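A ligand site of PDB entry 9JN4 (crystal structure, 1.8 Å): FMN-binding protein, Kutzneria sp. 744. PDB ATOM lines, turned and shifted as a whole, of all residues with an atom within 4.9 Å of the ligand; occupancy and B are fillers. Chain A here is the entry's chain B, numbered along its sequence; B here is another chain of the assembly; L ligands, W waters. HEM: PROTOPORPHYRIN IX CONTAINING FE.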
ATOM      1  N   LEU A  29      23.930 -14.067  -3.511  1.00  0.00           N
ATOM      2  CA  LEU A  29      24.911 -14.230  -4.614  1.00  0.00           C
ATOM      3  C   LEU A  29      26.003 -13.149  -4.422  1.00  0.00           C
ATOM      4  O   LEU A  29      25.918 -12.083  -4.997  1.00  0.00           O
ATOM      5  CB  LEU A  29      24.260 -14.228  -5.986  1.00  0.00           C
ATOM      6  CG  LEU A  29      25.198 -14.768  -7.100  1.00  0.00           C
ATOM      7  CD1 LEU A  29      25.441 -16.276  -6.945  1.00  0.00           C
ATOM      8  CD2 LEU A  29      24.753 -14.397  -8.516  1.00  0.00           C
ATOM      9  N   THR A  45      34.781 -14.372  -7.953  1.00  0.00           N
ATOM     10  CA  THR A  45      33.772 -15.371  -8.367  1.00  0.00           C
ATOM     11  C   THR A  45      32.443 -15.031  -7.701  1.00  0.00           C
ATOM     12  O   THR A  45      32.503 -14.733  -6.505  1.00  0.00           O
ATOM     13  CB  THR A  45      34.218 -16.785  -8.001  1.00  0.00           C
ATOM     14  OG1 THR A  45      35.466 -17.055  -8.653  1.00  0.00           O
ATOM     15  CG2 THR A  45      33.178 -17.791  -8.436  1.00  0.00           C
ATOM     16  N   HIS A  46      31.332 -15.047  -8.469  1.00  0.00           N
ATOM     17  CA  HIS A  46      29.964 -14.969  -7.868  1.00  0.00           C
ATOM     18  C   HIS A  46      29.570 -16.319  -7.271  1.00  0.00           C
ATOM     19  O   HIS A  46      29.572 -17.302  -7.968  1.00  0.00           O
ATOM     20  CB  HIS A  46      28.901 -14.525  -8.836  1.00  0.00           C
ATOM     21  CG  HIS A  46      28.908 -13.054  -9.128  1.00  0.00           C
ATOM     22  ND1 HIS A  46      29.730 -12.521 -10.090  1.00  0.00           N
ATOM     23  CD2 HIS A  46      28.127 -12.047  -8.660  1.00  0.00           C
ATOM     24  CE1 HIS A  46      29.519 -11.219 -10.159  1.00  0.00           C
ATOM     25  NE2 HIS A  46      28.514 -10.906  -9.303  1.00  0.00           N
ATOM     26  N   VAL A  47      29.320 -16.338  -5.977  1.00  0.00           N
ATOM     27  CA  VAL A  47      29.103 -17.597  -5.205  1.00  0.00           C
ATOM     28  C   VAL A  47      27.953 -17.351  -4.269  1.00  0.00           C
ATOM     29  O   VAL A  47      27.865 -16.253  -3.676  1.00  0.00           O
ATOM     30  CB  VAL A  47      30.362 -18.031  -4.400  1.00  0.00           C
ATOM     31  CG1 VAL A  47      31.509 -18.344  -5.315  1.00  0.00           C
ATOM     32  CG2 VAL A  47      30.774 -16.971  -3.385  1.00  0.00           C
ATOM     33  N   PRO A  48      27.096 -18.390  -4.112  1.00  0.00           N
ATOM     34  CA  PRO A  48      25.991 -18.356  -3.168  1.00  0.00           C
ATOM     35  C   PRO A  48      26.487 -18.600  -1.768  1.00  0.00           C
ATOM     36  O   PRO A  48      27.171 -19.638  -1.485  1.00  0.00           O
ATOM     37  CB  PRO A  48      25.068 -19.494  -3.629  1.00  0.00           C
ATOM     38  CG  PRO A  48      26.037 -20.498  -4.199  1.00  0.00           C
ATOM     39  CD  PRO A  48      27.133 -19.667  -4.828  1.00  0.00           C
ATOM     40  N   HIS A  70      29.458 -22.341  -1.632  1.00  0.00           N
ATOM     41  CA  HIS A  70      30.121 -23.292  -2.557  1.00  0.00           C
ATOM     42  C   HIS A  70      30.492 -22.570  -3.849  1.00  0.00           C
ATOM     43  O   HIS A  70      29.982 -21.450  -4.111  1.00  0.00           O
ATOM     44  CB  HIS A  70      29.285 -24.527  -2.843  1.00  0.00           C
ATOM     45  CG  HIS A  70      28.026 -24.351  -3.641  1.00  0.00           C
ATOM     46  ND1 HIS A  70      26.845 -23.867  -3.086  1.00  0.00           N
ATOM     47  CD2 HIS A  70      27.734 -24.789  -4.884  1.00  0.00           C
ATOM     48  CE1 HIS A  70      25.879 -23.916  -3.967  1.00  0.00           C
ATOM     49  NE2 HIS A  70      26.405 -24.516  -5.134  1.00  0.00           N
ATOM     50  N   MET A  71      31.319 -23.237  -4.635  1.00  0.00           N
ATOM     51  CA  MET A  71      31.755 -22.765  -5.946  1.00  0.00           C
ATOM     52  C   MET A  71      32.137 -24.009  -6.757  1.00  0.00           C
ATOM     53  O   MET A  71      31.957 -25.140  -6.257  1.00  0.00           O
ATOM     54  CB  MET A  71      32.920 -21.777  -5.837  1.00  0.00           C
ATOM     55  CG  MET A  71      34.206 -22.403  -5.418  1.00  0.00           C
ATOM     56  SD  MET A  71      35.534 -21.153  -5.602  1.00  0.00           S
ATOM     57  CE  MET A  71      35.495 -20.596  -3.927  1.00  0.00           C
ATOM     58  N   ASN A  72      32.535 -23.810  -7.990  1.00  0.00           N
ATOM     59  CA  ASN A  72      32.910 -24.920  -8.907  1.00  0.00           C
ATOM     60  C   ASN A  72      34.368 -25.289  -8.612  1.00  0.00           C
ATOM     61  O   ASN A  72      35.208 -24.396  -8.646  1.00  0.00           O
ATOM     62  CB  ASN A  72      32.604 -24.451 -10.318  1.00  0.00           C
ATOM     63  CG  ASN A  72      32.868 -25.504 -11.352  1.00  0.00           C
ATOM     64  OD1 ASN A  72      33.250 -26.621 -11.028  1.00  0.00           O
ATOM     65  ND2 ASN A  72      32.544 -25.146 -12.573  1.00  0.00           N
ATOM     66  N   ASN A  75      36.810 -24.269 -11.316  1.00  0.00           N
ATOM     67  CA  ASN A  75      37.152 -22.826 -11.325  1.00  0.00           C
ATOM     68  C   ASN A  75      38.576 -22.664 -10.762  1.00  0.00           C
ATOM     69  O   ASN A  75      38.852 -23.042  -9.628  1.00  0.00           O
ATOM     70  CB  ASN A  75      36.062 -22.037 -10.593  1.00  0.00           C
ATOM     71  CG  ASN A  75      36.298 -20.544 -10.591  1.00  0.00           C
ATOM     72  OD1 ASN A  75      37.406 -20.078 -10.914  1.00  0.00           O
ATOM     73  ND2 ASN A  75      35.264 -19.813 -10.234  1.00  0.00           N
ATOM     74  N   VAL A 136      25.079 -27.793   0.176  1.00  0.00           N
ATOM     75  CA  VAL A 136      24.127 -27.521  -0.942  1.00  0.00           C
ATOM     76  C   VAL A 136      22.665 -27.696  -0.482  1.00  0.00           C
ATOM     77  O   VAL A 136      21.836 -26.844  -0.863  1.00  0.00           O
ATOM     78  CB  VAL A 136      24.415 -28.328  -2.239  1.00  0.00           C
ATOM     79  CG1 VAL A 136      25.782 -28.037  -2.823  1.00  0.00           C
ATOM     80  CG2 VAL A 136      24.219 -29.800  -2.039  1.00  0.00           C
ATOM     81  N   THR A 139      21.670 -24.696   1.490  1.00  0.00           N
ATOM     82  CA  THR A 139      21.547 -23.554   0.560  1.00  0.00           C
ATOM     83  C   THR A 139      20.171 -23.645  -0.140  1.00  0.00           C
ATOM     84  O   THR A 139      19.471 -22.626  -0.207  1.00  0.00           O
ATOM     85  CB  THR A 139      22.722 -23.473  -0.410  1.00  0.00           C
ATOM     86  OG1 THR A 139      23.964 -23.346   0.304  1.00  0.00           O
ATOM     87  CG2 THR A 139      22.558 -22.319  -1.383  1.00  0.00           C
ATOM     88  N   VAL A 140      19.776 -24.829  -0.616  1.00  0.00           N
ATOM     89  CA  VAL A 140      18.399 -24.998  -1.182  1.00  0.00           C
ATOM     90  C   VAL A 140      17.397 -24.538  -0.118  1.00  0.00           C
ATOM     91  O   VAL A 140      16.435 -23.789  -0.466  1.00  0.00           O
ATOM     92  CB  VAL A 140      18.132 -26.435  -1.632  1.00  0.00           C
ATOM     93  CG1 VAL A 140      16.686 -26.608  -2.076  1.00  0.00           C
ATOM     94  CG2 VAL A 140      19.063 -26.833  -2.772  1.00  0.00           C
ATOM     95  N   LEU A 143      17.414 -20.742   0.273  1.00  0.00           N
ATOM     96  CA  LEU A 143      17.119 -19.879  -0.907  1.00  0.00           C
ATOM     97  C   LEU A 143      15.739 -20.245  -1.486  1.00  0.00           C
ATOM     98  O   LEU A 143      15.034 -19.314  -1.935  1.00  0.00           O
ATOM     99  CB  LEU A 143      18.171 -19.964  -2.013  1.00  0.00           C
ATOM    100  CG  LEU A 143      19.630 -19.610  -1.698  1.00  0.00           C
ATOM    101  CD1 LEU A 143      20.375 -19.193  -2.944  1.00  0.00           C
ATOM    102  CD2 LEU A 143      19.830 -18.667  -0.538  1.00  0.00           C
ATOM    103  N   PHE A 160      21.393 -34.898  -6.047  1.00  0.00           N
ATOM    104  CA  PHE A 160      22.442 -34.035  -5.452  1.00  0.00           C
ATOM    105  C   PHE A 160      23.698 -34.877  -5.213  1.00  0.00           C
ATOM    106  O   PHE A 160      24.795 -34.375  -5.459  1.00  0.00           O
ATOM    107  CB  PHE A 160      21.998 -33.434  -4.121  1.00  0.00           C
ATOM    108  CG  PHE A 160      20.882 -32.422  -4.176  1.00  0.00           C
ATOM    109  CD1 PHE A 160      20.323 -31.984  -5.369  1.00  0.00           C
ATOM    110  CD2 PHE A 160      20.411 -31.850  -3.003  1.00  0.00           C
ATOM    111  CE1 PHE A 160      19.300 -31.051  -5.396  1.00  0.00           C
ATOM    112  CE2 PHE A 160      19.417 -30.883  -3.021  1.00  0.00           C
ATOM    113  CZ  PHE A 160      18.845 -30.484  -4.225  1.00  0.00           C
ATOM    114  N   ILE A 163      25.564 -35.792  -8.503  1.00  0.00           N
ATOM    115  CA  ILE A 163      26.219 -34.656  -9.237  1.00  0.00           C
ATOM    116  C   ILE A 163      27.182 -33.890  -8.289  1.00  0.00           C
ATOM    117  O   ILE A 163      27.609 -32.794  -8.666  1.00  0.00           O
ATOM    118  CB  ILE A 163      25.204 -33.696  -9.873  1.00  0.00           C
ATOM    119  CG1 ILE A 163      24.272 -33.057  -8.840  1.00  0.00           C
ATOM    120  CG2 ILE A 163      24.415 -34.322 -10.975  1.00  0.00           C
ATOM    121  CD1 ILE A 163      23.776 -31.720  -9.252  1.00  0.00           C
ATOM    122  N   LEU A 164      27.589 -34.463  -7.173  1.00  0.00           N
ATOM    123  CA  LEU A 164      28.305 -33.750  -6.070  1.00  0.00           C
ATOM    124  C   LEU A 164      29.780 -33.439  -6.292  1.00  0.00           C
ATOM    125  O   LEU A 164      30.294 -32.528  -5.659  1.00  0.00           O
ATOM    126  CB  LEU A 164      28.152 -34.548  -4.773  1.00  0.00           C
ATOM    127  CG  LEU A 164      28.434 -33.807  -3.468  1.00  0.00           C
ATOM    128  CD1 LEU A 164      27.359 -32.767  -3.139  1.00  0.00           C
ATOM    129  CD2 LEU A 164      28.535 -34.777  -2.307  1.00  0.00           C
ATOM    130  N   GLY A 166      31.799 -31.957  -8.222  1.00  0.00           N
ATOM    131  CA  GLY A 166      32.119 -30.652  -8.822  1.00  0.00           C
ATOM    132  C   GLY A 166      31.977 -29.532  -7.788  1.00  0.00           C
ATOM    133  O   GLY A 166      32.572 -28.483  -7.961  1.00  0.00           O
ATOM    134  N   VAL A 167      31.230 -29.763  -6.697  1.00  0.00           N
ATOM    135  CA  VAL A 167      31.041 -28.731  -5.626  1.00  0.00           C
ATOM    136  C   VAL A 167      32.315 -28.523  -4.804  1.00  0.00           C
ATOM    137  O   VAL A 167      32.835 -29.519  -4.235  1.00  0.00           O
ATOM    138  CB  VAL A 167      29.873 -29.119  -4.702  1.00  0.00           C
ATOM    139  CG1 VAL A 167      29.635 -28.110  -3.599  1.00  0.00           C
ATOM    140  CG2 VAL A 167      28.635 -29.370  -5.525  1.00  0.00           C
ATOM    141  N   PHE B   7      36.749 -17.191 -14.757  1.00  0.00           N
ATOM    142  CA  PHE B   7      36.296 -18.536 -15.170  1.00  0.00           C
ATOM    143  C   PHE B   7      34.877 -18.407 -15.725  1.00  0.00           C
ATOM    144  O   PHE B   7      33.982 -17.990 -14.985  1.00  0.00           O
ATOM    145  CB  PHE B   7      36.231 -19.489 -13.977  1.00  0.00           C
ATOM    146  CG  PHE B   7      35.825 -20.867 -14.412  1.00  0.00           C
ATOM    147  CD1 PHE B   7      36.596 -21.542 -15.344  1.00  0.00           C
ATOM    148  CD2 PHE B   7      34.678 -21.452 -13.929  1.00  0.00           C
ATOM    149  CE1 PHE B   7      36.239 -22.815 -15.745  1.00  0.00           C
ATOM    150  CE2 PHE B   7      34.312 -22.723 -14.350  1.00  0.00           C
ATOM    151  CZ  PHE B   7      35.096 -23.397 -15.249  1.00  0.00           C
ATOM    152  N   TYR B  97      17.049 -15.722  -9.029  1.00  0.00           N
ATOM    153  CA  TYR B  97      17.040 -17.124  -8.571  1.00  0.00           C
ATOM    154  C   TYR B  97      16.189 -17.981  -9.500  1.00  0.00           C
ATOM    155  O   TYR B  97      15.113 -17.538  -9.885  1.00  0.00           O
ATOM    156  CB  TYR B  97      16.477 -17.187  -7.159  1.00  0.00           C
ATOM    157  CG  TYR B  97      16.366 -18.611  -6.664  1.00  0.00           C
ATOM    158  CD1 TYR B  97      17.445 -19.255  -6.121  1.00  0.00           C
ATOM    159  CD2 TYR B  97      15.145 -19.251  -6.598  1.00  0.00           C
ATOM    160  CE1 TYR B  97      17.348 -20.503  -5.531  1.00  0.00           C
ATOM    161  CE2 TYR B  97      15.017 -20.514  -6.048  1.00  0.00           C
ATOM    162  CZ  TYR B  97      16.137 -21.152  -5.524  1.00  0.00           C
ATOM    163  OH  TYR B  97      16.043 -22.359  -4.943  1.00  0.00           O
ATOM    164  N   ALA B 109      18.289 -29.361  -9.610  1.00  0.00           N
ATOM    165  CA  ALA B 109      18.844 -28.544  -8.516  1.00  0.00           C
ATOM    166  C   ALA B 109      18.589 -27.089  -8.872  1.00  0.00           C
ATOM    167  O   ALA B 109      18.557 -26.744 -10.046  1.00  0.00           O
ATOM    168  CB  ALA B 109      20.306 -28.870  -8.319  1.00  0.00           C
ATOM    169  N   PRO B 110      18.375 -26.196  -7.879  1.00  0.00           N
ATOM    170  CA  PRO B 110      18.216 -24.781  -8.184  1.00  0.00           C
ATOM    171  C   PRO B 110      19.535 -24.135  -8.656  1.00  0.00           C
ATOM    172  O   PRO B 110      20.583 -24.634  -8.417  1.00  0.00           O
ATOM    173  CB  PRO B 110      17.827 -24.134  -6.861  1.00  0.00           C
ATOM    174  CG  PRO B 110      17.460 -25.280  -5.954  1.00  0.00           C
ATOM    175  CD  PRO B 110      18.307 -26.453  -6.436  1.00  0.00           C
ATOM    176  N   THR B 111      19.459 -22.950  -9.228  1.00  0.00           N
ATOM    177  CA  THR B 111      20.663 -22.146  -9.493  1.00  0.00           C
ATOM    178  C   THR B 111      20.293 -20.655  -9.462  1.00  0.00           C
ATOM    179  O   THR B 111      19.150 -20.238  -9.015  1.00  0.00           O
ATOM    180  CB  THR B 111      21.314 -22.629 -10.782  1.00  0.00           C
ATOM    181  OG1 THR B 111      22.623 -22.053 -10.896  1.00  0.00           O
ATOM    182  CG2 THR B 111      20.541 -22.196 -12.000  1.00  0.00           C
ATOM    183  N   TRP B 112      21.267 -19.840  -9.791  1.00  0.00           N
ATOM    184  CA  TRP B 112      21.070 -18.386  -9.916  1.00  0.00           C
ATOM    185  C   TRP B 112      21.540 -17.958 -11.302  1.00  0.00           C
ATOM    186  O   TRP B 112      22.704 -18.191 -11.687  1.00  0.00           O
ATOM    187  CB  TRP B 112      21.761 -17.612  -8.781  1.00  0.00           C
ATOM    188  CG  TRP B 112      21.125 -16.296  -8.425  1.00  0.00           C
ATOM    189  CD1 TRP B 112      21.070 -15.164  -9.185  1.00  0.00           C
ATOM    190  CD2 TRP B 112      20.427 -15.979  -7.225  1.00  0.00           C
ATOM    191  NE1 TRP B 112      20.414 -14.157  -8.518  1.00  0.00           N
ATOM    192  CE2 TRP B 112      20.017 -14.623  -7.299  1.00  0.00           C
ATOM    193  CE3 TRP B 112      20.152 -16.693  -6.048  1.00  0.00           C
ATOM    194  CZ2 TRP B 112      19.315 -13.983  -6.273  1.00  0.00           C
ATOM    195  CZ3 TRP B 112      19.454 -16.060  -5.029  1.00  0.00           C
ATOM    196  CH2 TRP B 112      18.991 -14.738  -5.164  1.00  0.00           C
ATOM    197  N   PHE B 114      22.622 -15.056 -13.704  1.00  0.00           N
ATOM    198  CA  PHE B 114      23.263 -13.773 -13.459  1.00  0.00           C
ATOM    199  C   PHE B 114      24.153 -13.410 -14.635  1.00  0.00           C
ATOM    200  O   PHE B 114      24.530 -14.270 -15.535  1.00  0.00           O
ATOM    201  CB  PHE B 114      24.036 -13.801 -12.143  1.00  0.00           C
ATOM    202  CG  PHE B 114      25.374 -14.468 -12.175  1.00  0.00           C
ATOM    203  CD1 PHE B 114      25.498 -15.819 -11.888  1.00  0.00           C
ATOM    204  CD2 PHE B 114      26.539 -13.716 -12.345  1.00  0.00           C
ATOM    205  CE1 PHE B 114      26.740 -16.429 -11.869  1.00  0.00           C
ATOM    206  CE2 PHE B 114      27.772 -14.351 -12.364  1.00  0.00           C
ATOM    207  CZ  PHE B 114      27.866 -15.707 -12.158  1.00  0.00           C
ATOM    208  N   MET B 180      30.363 -13.387 -17.956  1.00  0.00           N
ATOM    209  CA  MET B 180      29.458 -14.470 -17.512  1.00  0.00           C
ATOM    210  C   MET B 180      28.045 -14.108 -17.943  1.00  0.00           C
ATOM    211  O   MET B 180      27.476 -13.080 -17.421  1.00  0.00           O
ATOM    212  CB  MET B 180      29.543 -14.619 -15.981  1.00  0.00           C
ATOM    213  CG  MET B 180      28.657 -15.697 -15.415  1.00  0.00           C
ATOM    214  SD  MET B 180      29.275 -17.372 -15.718  1.00  0.00           S
ATOM    215  CE  MET B 180      30.629 -17.362 -14.550  1.00  0.00           C
ATOM    216  N   LYS B 182      25.108 -16.207 -17.499  1.00  0.00           N
ATOM    217  CA  LYS B 182      24.614 -17.482 -16.958  1.00  0.00           C
ATOM    218  C   LYS B 182      23.088 -17.424 -17.063  1.00  0.00           C
ATOM    219  O   LYS B 182      22.422 -16.779 -16.203  1.00  0.00           O
ATOM    220  CB  LYS B 182      25.078 -17.671 -15.523  1.00  0.00           C
ATOM    221  CG  LYS B 182      24.593 -18.985 -14.940  1.00  0.00           C
ATOM    222  CD  LYS B 182      25.392 -19.434 -13.755  1.00  0.00           C
ATOM    223  CE  LYS B 182      24.612 -20.337 -12.820  1.00  0.00           C
ATOM    224  NZ  LYS B 182      23.862 -21.390 -13.543  1.00  0.00           N
HETATM  225  CHA HEM L   1      28.506 -24.301  -8.826  1.00  0.00           C
HETATM  226  CHB HEM L   1      24.876 -21.420  -7.361  1.00  0.00           C
HETATM  227  CHC HEM L   1      22.495 -25.222  -5.401  1.00  0.00           C
HETATM  228  CHD HEM L   1      25.828 -28.159  -7.388  1.00  0.00           C
HETATM  229  C1A HEM L   1      27.735 -23.200  -8.505  1.00  0.00           C
HETATM  230  C2A HEM L   1      28.029 -21.872  -8.991  1.00  0.00           C
HETATM  231  C3A HEM L   1      27.018 -21.057  -8.604  1.00  0.00           C
HETATM  232  C4A HEM L   1      26.058 -21.868  -7.909  1.00  0.00           C
HETATM  233  CMA HEM L   1      26.990 -19.568  -8.942  1.00  0.00           C
HETATM  234  CAA HEM L   1      29.266 -21.400  -9.778  1.00  0.00           C
HETATM  235  CBA HEM L   1      30.378 -20.961  -8.841  1.00  0.00           C
HETATM  236  CGA HEM L   1      31.663 -20.745  -9.636  1.00  0.00           C
HETATM  237  O1A HEM L   1      31.654 -20.013 -10.699  1.00  0.00           O
HETATM  238  O2A HEM L   1      32.754 -21.239  -9.222  1.00  0.00           O
HETATM  239  C1B HEM L   1      23.931 -22.209  -6.681  1.00  0.00           C
HETATM  240  C2B HEM L   1      22.723 -21.681  -6.165  1.00  0.00           C
HETATM  241  C3B HEM L   1      22.037 -22.730  -5.590  1.00  0.00           C
HETATM  242  C4B HEM L   1      22.840 -23.927  -5.833  1.00  0.00           C
HETATM  243  CMB HEM L   1      22.250 -20.231  -6.167  1.00  0.00           C
HETATM  244  CAB HEM L   1      20.773 -22.521  -4.870  1.00  0.00           C
HETATM  245  CBB HEM L   1      20.204 -23.347  -4.027  1.00  0.00           C
HETATM  246  C1C HEM L   1      23.173 -26.328  -5.757  1.00  0.00           C
HETATM  247  C2C HEM L   1      22.829 -27.622  -5.354  1.00  0.00           C
HETATM  248  C3C HEM L   1      23.757 -28.493  -5.983  1.00  0.00           C
HETATM  249  C4C HEM L   1      24.746 -27.669  -6.651  1.00  0.00           C
HETATM  250  CMC HEM L   1      21.632 -27.978  -4.532  1.00  0.00           C
HETATM  251  CAC HEM L   1      23.775 -29.915  -5.730  1.00  0.00           C
HETATM  252  CBC HEM L   1      24.838 -30.711  -5.792  1.00  0.00           C
HETATM  253  C1D HEM L   1      26.790 -27.322  -7.962  1.00  0.00           C
HETATM  254  C2D HEM L   1      27.893 -27.859  -8.747  1.00  0.00           C
HETATM  255  C3D HEM L   1      28.625 -26.830  -9.122  1.00  0.00           C
HETATM  256  C4D HEM L   1      27.987 -25.593  -8.572  1.00  0.00           C
HETATM  257  CMD HEM L   1      28.261 -29.328  -9.034  1.00  0.00           C
HETATM  258  CAD HEM L   1      29.926 -26.896  -9.925  1.00  0.00           C
HETATM  259  CBD HEM L   1      29.696 -26.361 -11.383  1.00  0.00           C
HETATM  260  CGD HEM L   1      28.428 -26.871 -12.051  1.00  0.00           C
HETATM  261  O1D HEM L   1      28.336 -28.110 -12.244  1.00  0.00           O
HETATM  262  O2D HEM L   1      27.465 -26.086 -12.361  1.00  0.00           O
HETATM  263  NA  HEM L   1      26.503 -23.175  -7.883  1.00  0.00           N
HETATM  264  NB  HEM L   1      23.980 -23.540  -6.401  1.00  0.00           N
HETATM  265  NC  HEM L   1      24.350 -26.350  -6.506  1.00  0.00           N
HETATM  266  ND  HEM L   1      26.846 -25.936  -7.886  1.00  0.00           N
HETATM  267 FE   HEM L   1      25.542 -24.747  -7.052  1.00  0.00          FE
HETATM  268  O   HOH W   1      26.593 -23.494 -11.796  1.00  0.00           O
HETATM  269  O   HOH W   2      25.630 -25.781 -14.524  1.00  0.00           O
HETATM  270  O   HOH W   3      29.988 -17.959 -10.680  1.00  0.00           O
HETATM  271  O   HOH W   4      24.094 -24.275  -9.659  1.00  0.00           O
HETATM  272  O   HOH W   5      29.599 -32.235 -10.429  1.00  0.00           O
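A ring nitrogen (NE2) of His 70 is bound to an iron atom (FE) of the ligand, at 2.1 Å.
The side-chain amide nitrogen (ND2) of Asn 75 sits at hydrogen-bond distance from an oxygen (O2A) of the ligand, at 3.1 Å.
An oxygen (O2A) of the ligand is in hydrogen-bond range of the backbone NH (N) of Asn 72.
OG1 of Thr 45 sits at hydrogen-bond distance from ND2 of Asn 75 (3.2 Å).
OG1 of Thr 111 of chain B sits at hydrogen-bond distance from NZ of Lys 182 of chain B (3.0 Å).
Residues that only touch the ligand: Thr 45, His 46, Pro 48, Met 71, Val 136, Thr 139, Val 140, Leu 143, Phe 160, Ile 163, Gly 166, Val 167, Pro 110 of chain B, Thr 111 of chain B and Trp 112 of chain B.
18 residues have an atom within 4 Å of the ligand: Thr 45, His 46, Pro 48, His 70, Met 71, Asn 72, Asn 75, Val 136, Thr 139, Val 140, Leu 143, Phe 160, Ile 163, Gly 166, Val 167, Pro 110 of chain B, Thr 111 of chain B and Trp 112 of chain B.
Water W3 bridges an oxygen (O1A) of the ligand (2.6 Å) and the backbone carbonyl oxygen (O) of His 46 (2.8 Å).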
